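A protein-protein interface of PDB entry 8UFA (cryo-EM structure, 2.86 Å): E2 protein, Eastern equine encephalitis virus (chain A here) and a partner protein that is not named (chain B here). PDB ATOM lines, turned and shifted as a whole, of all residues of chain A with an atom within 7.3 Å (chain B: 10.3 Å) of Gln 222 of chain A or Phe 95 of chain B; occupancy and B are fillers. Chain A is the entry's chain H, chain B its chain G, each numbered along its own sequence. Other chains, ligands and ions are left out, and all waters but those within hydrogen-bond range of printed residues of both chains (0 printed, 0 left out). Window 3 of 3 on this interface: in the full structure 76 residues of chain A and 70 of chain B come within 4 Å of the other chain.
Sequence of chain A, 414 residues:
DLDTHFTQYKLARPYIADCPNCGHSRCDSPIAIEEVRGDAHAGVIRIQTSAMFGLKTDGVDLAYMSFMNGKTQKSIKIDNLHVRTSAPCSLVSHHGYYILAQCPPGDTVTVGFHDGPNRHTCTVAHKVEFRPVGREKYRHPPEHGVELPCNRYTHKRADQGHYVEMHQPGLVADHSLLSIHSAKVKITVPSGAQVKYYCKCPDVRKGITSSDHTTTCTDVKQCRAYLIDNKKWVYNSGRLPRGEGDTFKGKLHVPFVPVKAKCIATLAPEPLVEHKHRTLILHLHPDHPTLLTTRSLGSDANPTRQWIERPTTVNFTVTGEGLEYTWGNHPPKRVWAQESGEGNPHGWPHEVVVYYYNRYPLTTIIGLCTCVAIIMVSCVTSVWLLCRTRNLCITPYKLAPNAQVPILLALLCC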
ATOM      1  N   LEU A 178      16.750  26.704  27.331  1.00  0.00           N
ATOM      2  CA  LEU A 178      15.484  27.029  27.973  1.00  0.00           C
ATOM      3  C   LEU A 178      15.418  26.497  29.400  1.00  0.00           C
ATOM      4  O   LEU A 178      15.814  25.359  29.671  1.00  0.00           O
ATOM      5  CB  LEU A 178      14.329  26.448  27.156  1.00  0.00           C
ATOM      6  CG  LEU A 178      14.260  26.933  25.708  1.00  0.00           C
ATOM      7  CD1 LEU A 178      13.258  26.114  24.923  1.00  0.00           C
ATOM      8  CD2 LEU A 178      13.890  28.401  25.665  1.00  0.00           C
ATOM      9  N   VAL A 185       9.260  30.496  31.331  1.00  0.00           N
ATOM     10  CA  VAL A 185      10.346  30.007  30.490  1.00  0.00           C
ATOM     11  C   VAL A 185      11.369  31.113  30.265  1.00  0.00           C
ATOM     12  O   VAL A 185      11.034  32.206  29.793  1.00  0.00           O
ATOM     13  CB  VAL A 185       9.810  29.460  29.154  1.00  0.00           C
ATOM     14  CG1 VAL A 185      10.955  29.122  28.215  1.00  0.00           C
ATOM     15  CG2 VAL A 185       8.965  28.223  29.398  1.00  0.00           C
ATOM     16  N   TYR A 198      11.251  30.837  19.220  1.00  0.00           N
ATOM     17  CA  TYR A 198       9.897  30.810  18.672  1.00  0.00           C
ATOM     18  C   TYR A 198       9.011  30.084  19.674  1.00  0.00           C
ATOM     19  O   TYR A 198       9.167  28.876  19.880  1.00  0.00           O
ATOM     20  CB  TYR A 198       9.863  30.115  17.310  1.00  0.00           C
ATOM     21  CG  TYR A 198       8.481  30.021  16.695  1.00  0.00           C
ATOM     22  CD1 TYR A 198       7.926  31.093  16.018  1.00  0.00           C
ATOM     23  CD2 TYR A 198       7.731  28.861  16.807  1.00  0.00           C
ATOM     24  CE1 TYR A 198       6.665  31.012  15.467  1.00  0.00           C
ATOM     25  CE2 TYR A 198       6.470  28.772  16.260  1.00  0.00           C
ATOM     26  CZ  TYR A 198       5.942  29.848  15.590  1.00  0.00           C
ATOM     27  OH  TYR A 198       4.691  29.752  15.030  1.00  0.00           O
ATOM     28  N   CYS A 199       8.082  30.811  20.288  1.00  0.00           N
ATOM     29  CA  CYS A 199       7.175  30.268  21.289  1.00  0.00           C
ATOM     30  C   CYS A 199       5.745  30.410  20.791  1.00  0.00           C
ATOM     31  O   CYS A 199       5.359  31.483  20.316  1.00  0.00           O
ATOM     32  CB  CYS A 199       7.327  31.002  22.621  1.00  0.00           C
ATOM     33  SG  CYS A 199       8.950  30.880  23.395  1.00  0.00           S
ATOM     34  N   LYS A 200       4.963  29.339  20.897  1.00  0.00           N
ATOM     35  CA  LYS A 200       3.581  29.346  20.429  1.00  0.00           C
ATOM     36  C   LYS A 200       2.637  28.836  21.511  1.00  0.00           C
ATOM     37  O   LYS A 200       1.769  27.995  21.272  1.00  0.00           O
ATOM     38  CB  LYS A 200       3.439  28.530  19.151  1.00  0.00           C
ATOM     39  CG  LYS A 200       2.140  28.770  18.404  1.00  0.00           C
ATOM     40  CD  LYS A 200       2.099  27.992  17.098  1.00  0.00           C
ATOM     41  CE  LYS A 200       0.825  28.286  16.324  1.00  0.00           C
ATOM     42  NZ  LYS A 200       0.775  27.558  15.030  1.00  0.00           N
ATOM     43  N   CYS A 201       2.810  29.334  22.726  1.00  0.00           N
ATOM     44  CA  CYS A 201       1.850  29.104  23.797  1.00  0.00           C
ATOM     45  C   CYS A 201       0.720  30.109  23.588  1.00  0.00           C
ATOM     46  O   CYS A 201       0.722  30.862  22.610  1.00  0.00           O
ATOM     47  CB  CYS A 201       2.559  29.187  25.149  1.00  0.00           C
ATOM     48  SG  CYS A 201       3.170  30.808  25.651  1.00  0.00           S
ATOM     49  N   PRO A 202      -0.286  30.147  24.472  1.00  0.00           N
ATOM     50  CA  PRO A 202      -1.385  31.104  24.250  1.00  0.00           C
ATOM     51  C   PRO A 202      -0.909  32.507  23.905  1.00  0.00           C
ATOM     52  O   PRO A 202      -1.550  33.193  23.100  1.00  0.00           O
ATOM     53  CB  PRO A 202      -2.147  31.063  25.579  1.00  0.00           C
ATOM     54  CG  PRO A 202      -1.922  29.687  26.078  1.00  0.00           C
ATOM     55  CD  PRO A 202      -0.506  29.359  25.698  1.00  0.00           C
ATOM     56  N   ARG A 205       5.111  34.402  21.006  1.00  0.00           N
ATOM     57  CA  ARG A 205       6.244  35.317  21.027  1.00  0.00           C
ATOM     58  C   ARG A 205       7.402  34.732  20.230  1.00  0.00           C
ATOM     59  O   ARG A 205       7.662  33.528  20.291  1.00  0.00           O
ATOM     60  CB  ARG A 205       6.705  35.601  22.461  1.00  0.00           C
ATOM     61  CG  ARG A 205       5.662  36.253  23.350  1.00  0.00           C
ATOM     62  CD  ARG A 205       5.360  37.675  22.908  1.00  0.00           C
ATOM     63  NE  ARG A 205       4.409  38.336  23.794  1.00  0.00           N
ATOM     64  CZ  ARG A 205       3.090  38.250  23.697  1.00  0.00           C
ATOM     65  NH1 ARG A 205       2.508  37.550  22.736  1.00  0.00           N
ATOM     66  NH2 ARG A 205       2.334  38.907  24.572  1.00  0.00           N
ATOM     67  N   THR A 216       6.516  34.630  28.166  1.00  0.00           N
ATOM     68  CA  THR A 216       5.261  34.410  28.872  1.00  0.00           C
ATOM     69  C   THR A 216       4.868  32.942  28.997  1.00  0.00           C
ATOM     70  O   THR A 216       3.954  32.632  29.768  1.00  0.00           O
ATOM     71  CB  THR A 216       4.139  35.155  28.148  1.00  0.00           C
ATOM     72  OG1 THR A 216       4.110  34.742  26.776  1.00  0.00           O
ATOM     73  CG2 THR A 216       4.357  36.656  28.215  1.00  0.00           C
ATOM     74  N   CYS A 217       5.520  32.037  28.274  1.00  0.00           N
ATOM     75  CA  CYS A 217       5.175  30.626  28.357  1.00  0.00           C
ATOM     76  C   CYS A 217       5.729  30.017  29.641  1.00  0.00           C
ATOM     77  O   CYS A 217       6.728  30.484  30.196  1.00  0.00           O
ATOM     78  CB  CYS A 217       5.694  29.874  27.133  1.00  0.00           C
ATOM     79  SG  CYS A 217       5.196  30.626  25.553  1.00  0.00           S
ATOM     80  N   THR A 218       5.063  28.964  30.114  1.00  0.00           N
ATOM     81  CA  THR A 218       5.390  28.341  31.391  1.00  0.00           C
ATOM     82  C   THR A 218       6.002  26.954  31.268  1.00  0.00           C
ATOM     83  O   THR A 218       6.311  26.343  32.296  1.00  0.00           O
ATOM     84  CB  THR A 218       4.132  28.239  32.263  1.00  0.00           C
ATOM     85  OG1 THR A 218       3.159  27.417  31.605  1.00  0.00           O
ATOM     86  CG2 THR A 218       3.542  29.613  32.519  1.00  0.00           C
ATOM     87  N   ASP A 219       6.186  26.431  30.057  1.00  0.00           N
ATOM     88  CA  ASP A 219       6.788  25.115  29.893  1.00  0.00           C
ATOM     89  C   ASP A 219       7.770  25.146  28.733  1.00  0.00           C
ATOM     90  O   ASP A 219       7.491  25.733  27.684  1.00  0.00           O
ATOM     91  CB  ASP A 219       5.732  24.030  29.657  1.00  0.00           C
ATOM     92  CG  ASP A 219       6.303  22.632  29.774  1.00  0.00           C
ATOM     93  OD1 ASP A 219       7.543  22.502  29.862  1.00  0.00           O
ATOM     94  OD2 ASP A 219       5.516  21.663  29.792  1.00  0.00           O
ATOM     95  N   VAL A 220       8.921  24.505  28.939  1.00  0.00           N
ATOM     96  CA  VAL A 220       9.980  24.498  27.934  1.00  0.00           C
ATOM     97  C   VAL A 220       9.493  23.919  26.611  1.00  0.00           C
ATOM     98  O   VAL A 220       9.851  24.414  25.537  1.00  0.00           O
ATOM     99  CB  VAL A 220      11.199  23.722  28.463  1.00  0.00           C
ATOM    100  CG1 VAL A 220      12.195  23.473  27.344  1.00  0.00           C
ATOM    101  CG2 VAL A 220      11.851  24.482  29.603  1.00  0.00           C
ATOM    102  N   LYS A 221       8.666  22.871  26.657  1.00  0.00           N
ATOM    103  CA  LYS A 221       8.226  22.259  25.408  1.00  0.00           C
ATOM    104  C   LYS A 221       7.385  23.209  24.566  1.00  0.00           C
ATOM    105  O   LYS A 221       7.159  22.935  23.382  1.00  0.00           O
ATOM    106  CB  LYS A 221       7.472  20.951  25.678  1.00  0.00           C
ATOM    107  CG  LYS A 221       6.101  21.070  26.313  1.00  0.00           C
ATOM    108  CD  LYS A 221       5.465  19.687  26.379  1.00  0.00           C
ATOM    109  CE  LYS A 221       4.074  19.707  26.979  1.00  0.00           C
ATOM    110  NZ  LYS A 221       4.112  19.851  28.455  1.00  0.00           N
ATOM    111  N   GLN A 222       6.912  24.312  25.144  1.00  0.00           N
ATOM    112  CA  GLN A 222       6.131  25.288  24.397  1.00  0.00           C
ATOM    113  C   GLN A 222       6.994  26.210  23.546  1.00  0.00           C
ATOM    114  O   GLN A 222       6.446  26.967  22.737  1.00  0.00           O
ATOM    115  CB  GLN A 222       5.298  26.131  25.362  1.00  0.00           C
ATOM    116  CG  GLN A 222       4.309  25.324  26.183  1.00  0.00           C
ATOM    117  CD  GLN A 222       3.603  26.156  27.231  1.00  0.00           C
ATOM    118  OE1 GLN A 222       4.230  26.923  27.958  1.00  0.00           O
ATOM    119  NE2 GLN A 222       2.287  26.008  27.309  1.00  0.00           N
ATOM    120  N   CYS A 223       8.317  26.166  23.702  1.00  0.00           N
ATOM    121  CA  CYS A 223       9.223  27.042  22.974  1.00  0.00           C
ATOM    122  C   CYS A 223      10.301  26.232  22.267  1.00  0.00           C
ATOM    123  O   CYS A 223      10.595  25.089  22.630  1.00  0.00           O
ATOM    124  CB  CYS A 223       9.895  28.046  23.915  1.00  0.00           C
ATOM    125  SG  CYS A 223       8.802  29.282  24.637  1.00  0.00           S
ATOM    126  N   ARG A 224      10.890  26.850  21.244  1.00  0.00           N
ATOM    127  CA  ARG A 224      12.059  26.325  20.550  1.00  0.00           C
ATOM    128  C   ARG A 224      13.130  27.404  20.567  1.00  0.00           C
ATOM    129  O   ARG A 224      12.848  28.562  20.247  1.00  0.00           O
ATOM    130  CB  ARG A 224      11.738  25.929  19.105  1.00  0.00           C
ATOM    131  CG  ARG A 224      10.755  24.791  18.968  1.00  0.00           C
ATOM    132  CD  ARG A 224      11.338  23.478  19.438  1.00  0.00           C
ATOM    133  NE  ARG A 224      10.378  22.392  19.294  1.00  0.00           N
ATOM    134  CZ  ARG A 224       9.433  22.108  20.179  1.00  0.00           C
ATOM    135  NH1 ARG A 224       9.260  22.841  21.267  1.00  0.00           N
ATOM    136  NH2 ARG A 224       8.620  21.081  19.948  1.00  0.00           N
ATOM    137  N   TYR A 226      17.054  28.543  19.264  1.00  0.00           N
ATOM    138  CA  TYR A 226      18.079  28.351  18.250  1.00  0.00           C
ATOM    139  C   TYR A 226      19.276  29.228  18.581  1.00  0.00           C
ATOM    140  O   TYR A 226      19.118  30.398  18.939  1.00  0.00           O
ATOM    141  CB  TYR A 226      17.556  28.695  16.855  1.00  0.00           C
ATOM    142  CG  TYR A 226      16.279  27.986  16.483  1.00  0.00           C
ATOM    143  CD1 TYR A 226      16.306  26.751  15.860  1.00  0.00           C
ATOM    144  CD2 TYR A 226      15.048  28.555  16.749  1.00  0.00           C
ATOM    145  CE1 TYR A 226      15.145  26.108  15.506  1.00  0.00           C
ATOM    146  CE2 TYR A 226      13.880  27.920  16.403  1.00  0.00           C
ATOM    147  CZ  TYR A 226      13.933  26.696  15.781  1.00  0.00           C
ATOM    148  OH  TYR A 226      12.767  26.050  15.448  1.00  0.00           O
ATOM    149  N   VAL B  60      15.478  24.128   5.813  1.00  0.00           N
ATOM    150  CA  VAL B  60      14.439  23.595   6.685  1.00  0.00           C
ATOM    151  C   VAL B  60      13.622  24.779   7.184  1.00  0.00           C
ATOM    152  O   VAL B  60      14.113  25.608   7.960  1.00  0.00           O
ATOM    153  CB  VAL B  60      15.026  22.782   7.846  1.00  0.00           C
ATOM    154  CG1 VAL B  60      13.920  22.231   8.732  1.00  0.00           C
ATOM    155  CG2 VAL B  60      15.886  21.648   7.306  1.00  0.00           C
ATOM    156  N   LYS B  61      12.373  24.854   6.735  1.00  0.00           N
ATOM    157  CA  LYS B  61      11.462  25.943   7.065  1.00  0.00           C
ATOM    158  C   LYS B  61      10.498  25.461   8.141  1.00  0.00           C
ATOM    159  O   LYS B  61       9.665  24.584   7.890  1.00  0.00           O
ATOM    160  CB  LYS B  61      10.715  26.406   5.817  1.00  0.00           C
ATOM    161  CG  LYS B  61       9.660  27.469   6.052  1.00  0.00           C
ATOM    162  CD  LYS B  61      10.241  28.753   6.610  1.00  0.00           C
ATOM    163  CE  LYS B  61       9.149  29.797   6.775  1.00  0.00           C
ATOM    164  NZ  LYS B  61       9.639  31.057   7.386  1.00  0.00           N
ATOM    165  N   CYS B  62      10.611  26.031   9.335  1.00  0.00           N
ATOM    166  CA  CYS B  62       9.752  25.660  10.447  1.00  0.00           C
ATOM    167  C   CYS B  62       8.482  26.498  10.435  1.00  0.00           C
ATOM    168  O   CYS B  62       8.526  27.714  10.230  1.00  0.00           O
ATOM    169  CB  CYS B  62      10.474  25.857  11.780  1.00  0.00           C
ATOM    170  SG  CYS B  62      11.987  24.899  11.984  1.00  0.00           S
ATOM    171  N   CYS B  63       7.351  25.838  10.666  1.00  0.00           N
ATOM    172  CA  CYS B  63       6.050  26.500  10.693  1.00  0.00           C
ATOM    173  C   CYS B  63       5.820  27.320   9.424  1.00  0.00           C
ATOM    174  O   CYS B  63       5.461  28.499   9.466  1.00  0.00           O
ATOM    175  CB  CYS B  63       5.916  27.362  11.946  1.00  0.00           C
ATOM    176  SG  CYS B  63       5.978  26.401  13.483  1.00  0.00           S
ATOM    177  N   GLY B  64       6.029  26.678   8.281  1.00  0.00           N
ATOM    178  CA  GLY B  64       5.850  27.347   7.010  1.00  0.00           C
ATOM    179  C   GLY B  64       6.296  26.454   5.871  1.00  0.00           C
ATOM    180  O   GLY B  64       6.517  25.254   6.048  1.00  0.00           O
ATOM    181  N   VAL B  84       7.714  17.367   7.242  1.00  0.00           N
ATOM    182  CA  VAL B  84       8.907  16.825   7.883  1.00  0.00           C
ATOM    183  C   VAL B  84       8.977  17.342   9.312  1.00  0.00           C
ATOM    184  O   VAL B  84       8.507  18.442   9.613  1.00  0.00           O
ATOM    185  CB  VAL B  84      10.171  17.204   7.083  1.00  0.00           C
ATOM    186  CG1 VAL B  84      10.081  16.656   5.671  1.00  0.00           C
ATOM    187  CG2 VAL B  84      10.363  18.713   7.069  1.00  0.00           C
ATOM    188  N   TYR B  85       9.554  16.549  10.213  1.00  0.00           N
ATOM    189  CA  TYR B  85       9.752  16.962  11.605  1.00  0.00           C
ATOM    190  C   TYR B  85      11.143  16.530  12.048  1.00  0.00           C
ATOM    191  O   TYR B  85      11.309  15.559  12.793  1.00  0.00           O
ATOM    192  CB  TYR B  85       8.671  16.387  12.520  1.00  0.00           C
ATOM    193  CG  TYR B  85       8.603  17.120  13.836  1.00  0.00           C
ATOM    194  CD1 TYR B  85       8.011  18.368  13.914  1.00  0.00           C
ATOM    195  CD2 TYR B  85       9.139  16.580  14.988  1.00  0.00           C
ATOM    196  CE1 TYR B  85       7.926  19.043  15.104  1.00  0.00           C
ATOM    197  CE2 TYR B  85       9.077  17.256  16.184  1.00  0.00           C
ATOM    198  CZ  TYR B  85       8.467  18.489  16.239  1.00  0.00           C
ATOM    199  OH  TYR B  85       8.429  19.186  17.423  1.00  0.00           O
ATOM    200  N   PRO B  86      12.172  17.237  11.592  1.00  0.00           N
ATOM    201  CA  PRO B  86      13.549  16.821  11.876  1.00  0.00           C
ATOM    202  C   PRO B  86      13.984  17.033  13.318  1.00  0.00           C
ATOM    203  O   PRO B  86      13.493  17.915  14.025  1.00  0.00           O
ATOM    204  CB  PRO B  86      14.376  17.695  10.930  1.00  0.00           C
ATOM    205  CG  PRO B  86      13.548  18.881  10.677  1.00  0.00           C
ATOM    206  CD  PRO B  86      12.121  18.448  10.755  1.00  0.00           C
ATOM    207  N   PHE B  87      14.936  16.199  13.740  1.00  0.00           N
ATOM    208  CA  PHE B  87      15.575  16.272  15.046  1.00  0.00           C
ATOM    209  C   PHE B  87      17.079  16.420  14.866  1.00  0.00           C
ATOM    210  O   PHE B  87      17.647  15.974  13.865  1.00  0.00           O
ATOM    211  CB  PHE B  87      15.307  15.020  15.892  1.00  0.00           C
ATOM    212  CG  PHE B  87      13.887  14.871  16.332  1.00  0.00           C
ATOM    213  CD1 PHE B  87      12.958  14.258  15.520  1.00  0.00           C
ATOM    214  CD2 PHE B  87      13.490  15.318  17.576  1.00  0.00           C
ATOM    215  CE1 PHE B  87      11.656  14.112  15.931  1.00  0.00           C
ATOM    216  CE2 PHE B  87      12.192  15.172  17.994  1.00  0.00           C
ATOM    217  CZ  PHE B  87      11.270  14.566  17.172  1.00  0.00           C
ATOM    218  N   GLY B  91      17.559  18.389  19.954  1.00  0.00           N
ATOM    219  CA  GLY B  91      16.163  18.015  19.988  1.00  0.00           C
ATOM    220  C   GLY B  91      15.444  18.350  18.700  1.00  0.00           C
ATOM    221  O   GLY B  91      16.041  18.504  17.632  1.00  0.00           O
ATOM    222  N   ALA B  92      14.123  18.460  18.812  1.00  0.00           N
ATOM    223  CA  ALA B  92      13.309  18.802  17.656  1.00  0.00           C
ATOM    224  C   ALA B  92      13.729  20.154  17.094  1.00  0.00           C
ATOM    225  O   ALA B  92      13.831  21.143  17.826  1.00  0.00           O
ATOM    226  CB  ALA B  92      11.832  18.821  18.043  1.00  0.00           C
ATOM    227  N   TYR B  93      13.972  20.191  15.784  1.00  0.00           N
ATOM    228  CA  TYR B  93      14.403  21.429  15.145  1.00  0.00           C
ATOM    229  C   TYR B  93      13.261  22.430  15.029  1.00  0.00           C
ATOM    230  O   TYR B  93      13.442  23.621  15.311  1.00  0.00           O
ATOM    231  CB  TYR B  93      14.980  21.120  13.765  1.00  0.00           C
ATOM    232  CG  TYR B  93      15.567  22.319  13.059  1.00  0.00           C
ATOM    233  CD1 TYR B  93      16.800  22.829  13.424  1.00  0.00           C
ATOM    234  CD2 TYR B  93      14.900  22.920  12.006  1.00  0.00           C
ATOM    235  CE1 TYR B  93      17.341  23.913  12.780  1.00  0.00           C
ATOM    236  CE2 TYR B  93      15.434  24.003  11.354  1.00  0.00           C
ATOM    237  CZ  TYR B  93      16.655  24.497  11.743  1.00  0.00           C
ATOM    238  OH  TYR B  93      17.193  25.580  11.093  1.00  0.00           O
ATOM    239  N   CYS B  94      12.081  21.973  14.624  1.00  0.00           N
ATOM    240  CA  CYS B  94      10.932  22.837  14.403  1.00  0.00           C
ATOM    241  C   CYS B  94       9.856  22.621  15.459  1.00  0.00           C
ATOM    242  O   CYS B  94       9.750  21.555  16.067  1.00  0.00           O
ATOM    243  CB  CYS B  94      10.331  22.591  13.021  1.00  0.00           C
ATOM    244  SG  CYS B  94      11.407  22.987  11.624  1.00  0.00           S
ATOM    245  N   PHE B  95       9.049  23.664  15.663  1.00  0.00           N
ATOM    246  CA  PHE B  95       7.938  23.589  16.605  1.00  0.00           C
ATOM    247  C   PHE B  95       6.721  22.895  16.001  1.00  0.00           C
ATOM    248  O   PHE B  95       6.140  21.996  16.617  1.00  0.00           O
ATOM    249  CB  PHE B  95       7.548  24.993  17.066  1.00  0.00           C
ATOM    250  CG  PHE B  95       6.421  25.010  18.053  1.00  0.00           C
ATOM    251  CD1 PHE B  95       6.668  24.902  19.405  1.00  0.00           C
ATOM    252  CD2 PHE B  95       5.113  25.145  17.627  1.00  0.00           C
ATOM    253  CE1 PHE B  95       5.638  24.922  20.314  1.00  0.00           C
ATOM    254  CE2 PHE B  95       4.077  25.162  18.529  1.00  0.00           C
ATOM    255  CZ  PHE B  95       4.339  25.044  19.877  1.00  0.00           C
ATOM    256  N   CYS B  96       6.321  23.305  14.801  1.00  0.00           N
ATOM    257  CA  CYS B  96       5.113  22.771  14.188  1.00  0.00           C
ATOM    258  C   CYS B  96       5.315  21.330  13.732  1.00  0.00           C
ATOM    259  O   CYS B  96       6.354  20.975  13.170  1.00  0.00           O
ATOM    260  CB  CYS B  96       4.693  23.650  13.012  1.00  0.00           C
ATOM    261  SG  CYS B  96       4.239  25.345  13.485  1.00  0.00           S
ATOM    262  N   ASP B  97       4.297  20.501  13.976  1.00  0.00           N
ATOM    263  CA  ASP B  97       4.383  19.076  13.672  1.00  0.00           C
ATOM    264  C   ASP B  97       4.204  18.770  12.190  1.00  0.00           C
ATOM    265  O   ASP B  97       4.844  17.847  11.674  1.00  0.00           O
ATOM    266  CB  ASP B  97       3.328  18.314  14.477  1.00  0.00           C
ATOM    267  CG  ASP B  97       3.555  18.405  15.973  1.00  0.00           C
ATOM    268  OD1 ASP B  97       4.521  17.788  16.470  1.00  0.00           O
ATOM    269  OD2 ASP B  97       2.766  19.095  16.654  1.00  0.00           O
ATOM    270  N   THR B  98       3.350  19.517  11.493  1.00  0.00           N
ATOM    271  CA  THR B  98       3.060  19.262  10.088  1.00  0.00           C
ATOM    272  C   THR B  98       3.332  20.448   9.180  1.00  0.00           C
ATOM    273  O   THR B  98       3.694  20.242   8.021  1.00  0.00           O
ATOM    274  CB  THR B  98       1.594  18.833   9.913  1.00  0.00           C
ATOM    275  OG1 THR B  98       0.729  19.816  10.497  1.00  0.00           O
ATOM    276  CG2 THR B  98       1.352  17.486  10.570  1.00  0.00           C
ATOM    277  N   GLU B  99       3.178  21.677   9.671  1.00  0.00           N
ATOM    278  CA  GLU B  99       3.449  22.873   8.876  1.00  0.00           C
ATOM    279  C   GLU B  99       4.962  23.085   8.867  1.00  0.00           C
ATOM    280  O   GLU B  99       5.505  24.026   9.443  1.00  0.00           O
ATOM    281  CB  GLU B  99       2.709  24.078   9.440  1.00  0.00           C
ATOM    282  CG  GLU B  99       1.192  23.949   9.412  1.00  0.00           C
ATOM    283  CD  GLU B  99       0.653  23.066  10.521  1.00  0.00           C
ATOM    284  OE1 GLU B  99       1.466  22.430  11.225  1.00  0.00           O
ATOM    285  OE2 GLU B  99      -0.583  23.004  10.686  1.00  0.00           O
ATOM    286  N   ASN B 100       5.648  22.171   8.185  1.00  0.00           N
ATOM    287  CA  ASN B 100       7.102  22.114   8.237  1.00  0.00           C
ATOM    288  C   ASN B 100       7.627  21.591   6.909  1.00  0.00           C
ATOM    289  O   ASN B 100       7.165  20.553   6.427  1.00  0.00           O
ATOM    290  CB  ASN B 100       7.530  21.205   9.388  1.00  0.00           C
ATOM    291  CG  ASN B 100       9.006  21.243   9.641  1.00  0.00           C
ATOM    292  OD1 ASN B 100       9.785  21.686   8.800  1.00  0.00           O
ATOM    293  ND2 ASN B 100       9.404  20.805  10.825  1.00  0.00           N
ATOM    294  N   THR B 101       8.584  22.312   6.323  1.00  0.00           N
ATOM    295  CA  THR B 101       9.077  22.024   4.982  1.00  0.00           C
ATOM    296  C   THR B 101      10.599  21.966   4.914  1.00  0.00           C
ATOM    297  O   THR B 101      11.287  22.800   5.513  1.00  0.00           O
ATOM    298  CB  THR B 101       8.578  23.092   4.009  1.00  0.00           C
ATOM    299  OG1 THR B 101       7.146  23.130   4.032  1.00  0.00           O
ATOM    300  CG2 THR B 101       9.046  22.798   2.617  1.00  0.00           C
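SG of Cys 62 of chain B is in hydrogen-bond range of OH of Tyr 226 of chain A, at 3.7 Å. OH of Tyr 85 of chain B is in hydrogen-bond range of NH2 of Arg 224 of chain A. The side-chain hydroxyl (OH) of Tyr 226 of chain A sits at hydrogen-bond distance from the backbone carbonyl oxygen (O) of Tyr 93 of chain B (2.5 Å). The backbone carbonyl oxygen (O) of Cys 94 of chain B lies within hydrogen-bond range of the guanidinium group (NE) of Arg 224 of chain A (3.4 Å).
SG of Cys 94 of chain B sits close to ND2 of Asn 100 of chain B (3.1 Å). The backbone carbonyl oxygen (O) of Gln 222 of chain A lies within hydrogen-bond range of the backbone NH (N) of Lys 200 of chain A (3.3 Å). The side-chain amide oxygen (OE1) of Gln 222 of chain A lies within hydrogen-bond range of the backbone NH (N) of Thr 218 of chain A, 3.1 Å away. OD2 of Asp 219 of chain A lies within salt-bridge range of NZ of Lys 221 of chain A, 2.7 Å away. SG of Cys 199 of chain A is disulfide-bonded to SG of Cys 223 of chain A (2.0 Å).
Among the printed residues, merely in contact across the chains: Tyr 198 of chain A with Cys 63 of chain B (3.7 Å), Tyr 198 of chain A with Phe 95 of chain B (3.9 Å), Lys 200 of chain A with Phe 95 of chain B (3.5 Å), Lys 221 of chain A with Phe 95 of chain B (3.96 Å), Gln 222 of chain A with Phe 95 of chain B (3.3 Å), Arg 224 of chain A with Ala 92 of chain B (3.8 Å), Arg 224 of chain A with Phe 95 of chain B (3.7 Å) and Tyr 226 of chain A with Cys 94 of chain B (3.8 Å).
Cys 199 of chain A touches none of the printed residues of chain B. Lys 200 of chain A touches one residue of chain B. No residue of chain B comes within 4 Å of Cys 217 of chain A. No residue of chain B comes within 4 Å of Thr 218 of chain A. Of chain B, only Phe 95 comes within 4 Å of Lys 221 of chain A. Cys 223 of chain A touches none of the printed residues of chain B. Of the printed residues of chain B, Tyr 198 of chain A touches Cys 63 (3.7 Å) and Phe 95 (3.9 Å). Of the printed residues of chain B, Arg 224 of chain A touches Tyr 85 (3.2 Å), Ala 92 (3.8 Å), Cys 94 (3.4 Å) and Phe 95 (3.7 Å). Of the printed residues of chain B, Tyr 226 of chain A touches Cys 62, Tyr 93 and Cys 94. The nearest residue of chain A that does not touch Phe 95 of chain B is Tyr 226 of chain A (4.4 Å). The nearest printed residue of chain A that does not touch Tyr 93 of chain B is Arg 224 of chain A (4.6 Å).
Of the 18 printed residues of chain A, 6 touch a printed residue of chain B. Printed residues of chain B that touch a printed residue of chain A: Cys 62, Cys 63, Tyr 85, Ala 92, Tyr 93, Cys 94 and Phe 95. Hydrophobic or aromatic side chains of chain B within 4 Å of the printed part of chain A: Tyr 85 and Phe 95. Among the printed residues, 12 pairs touch across the chains.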
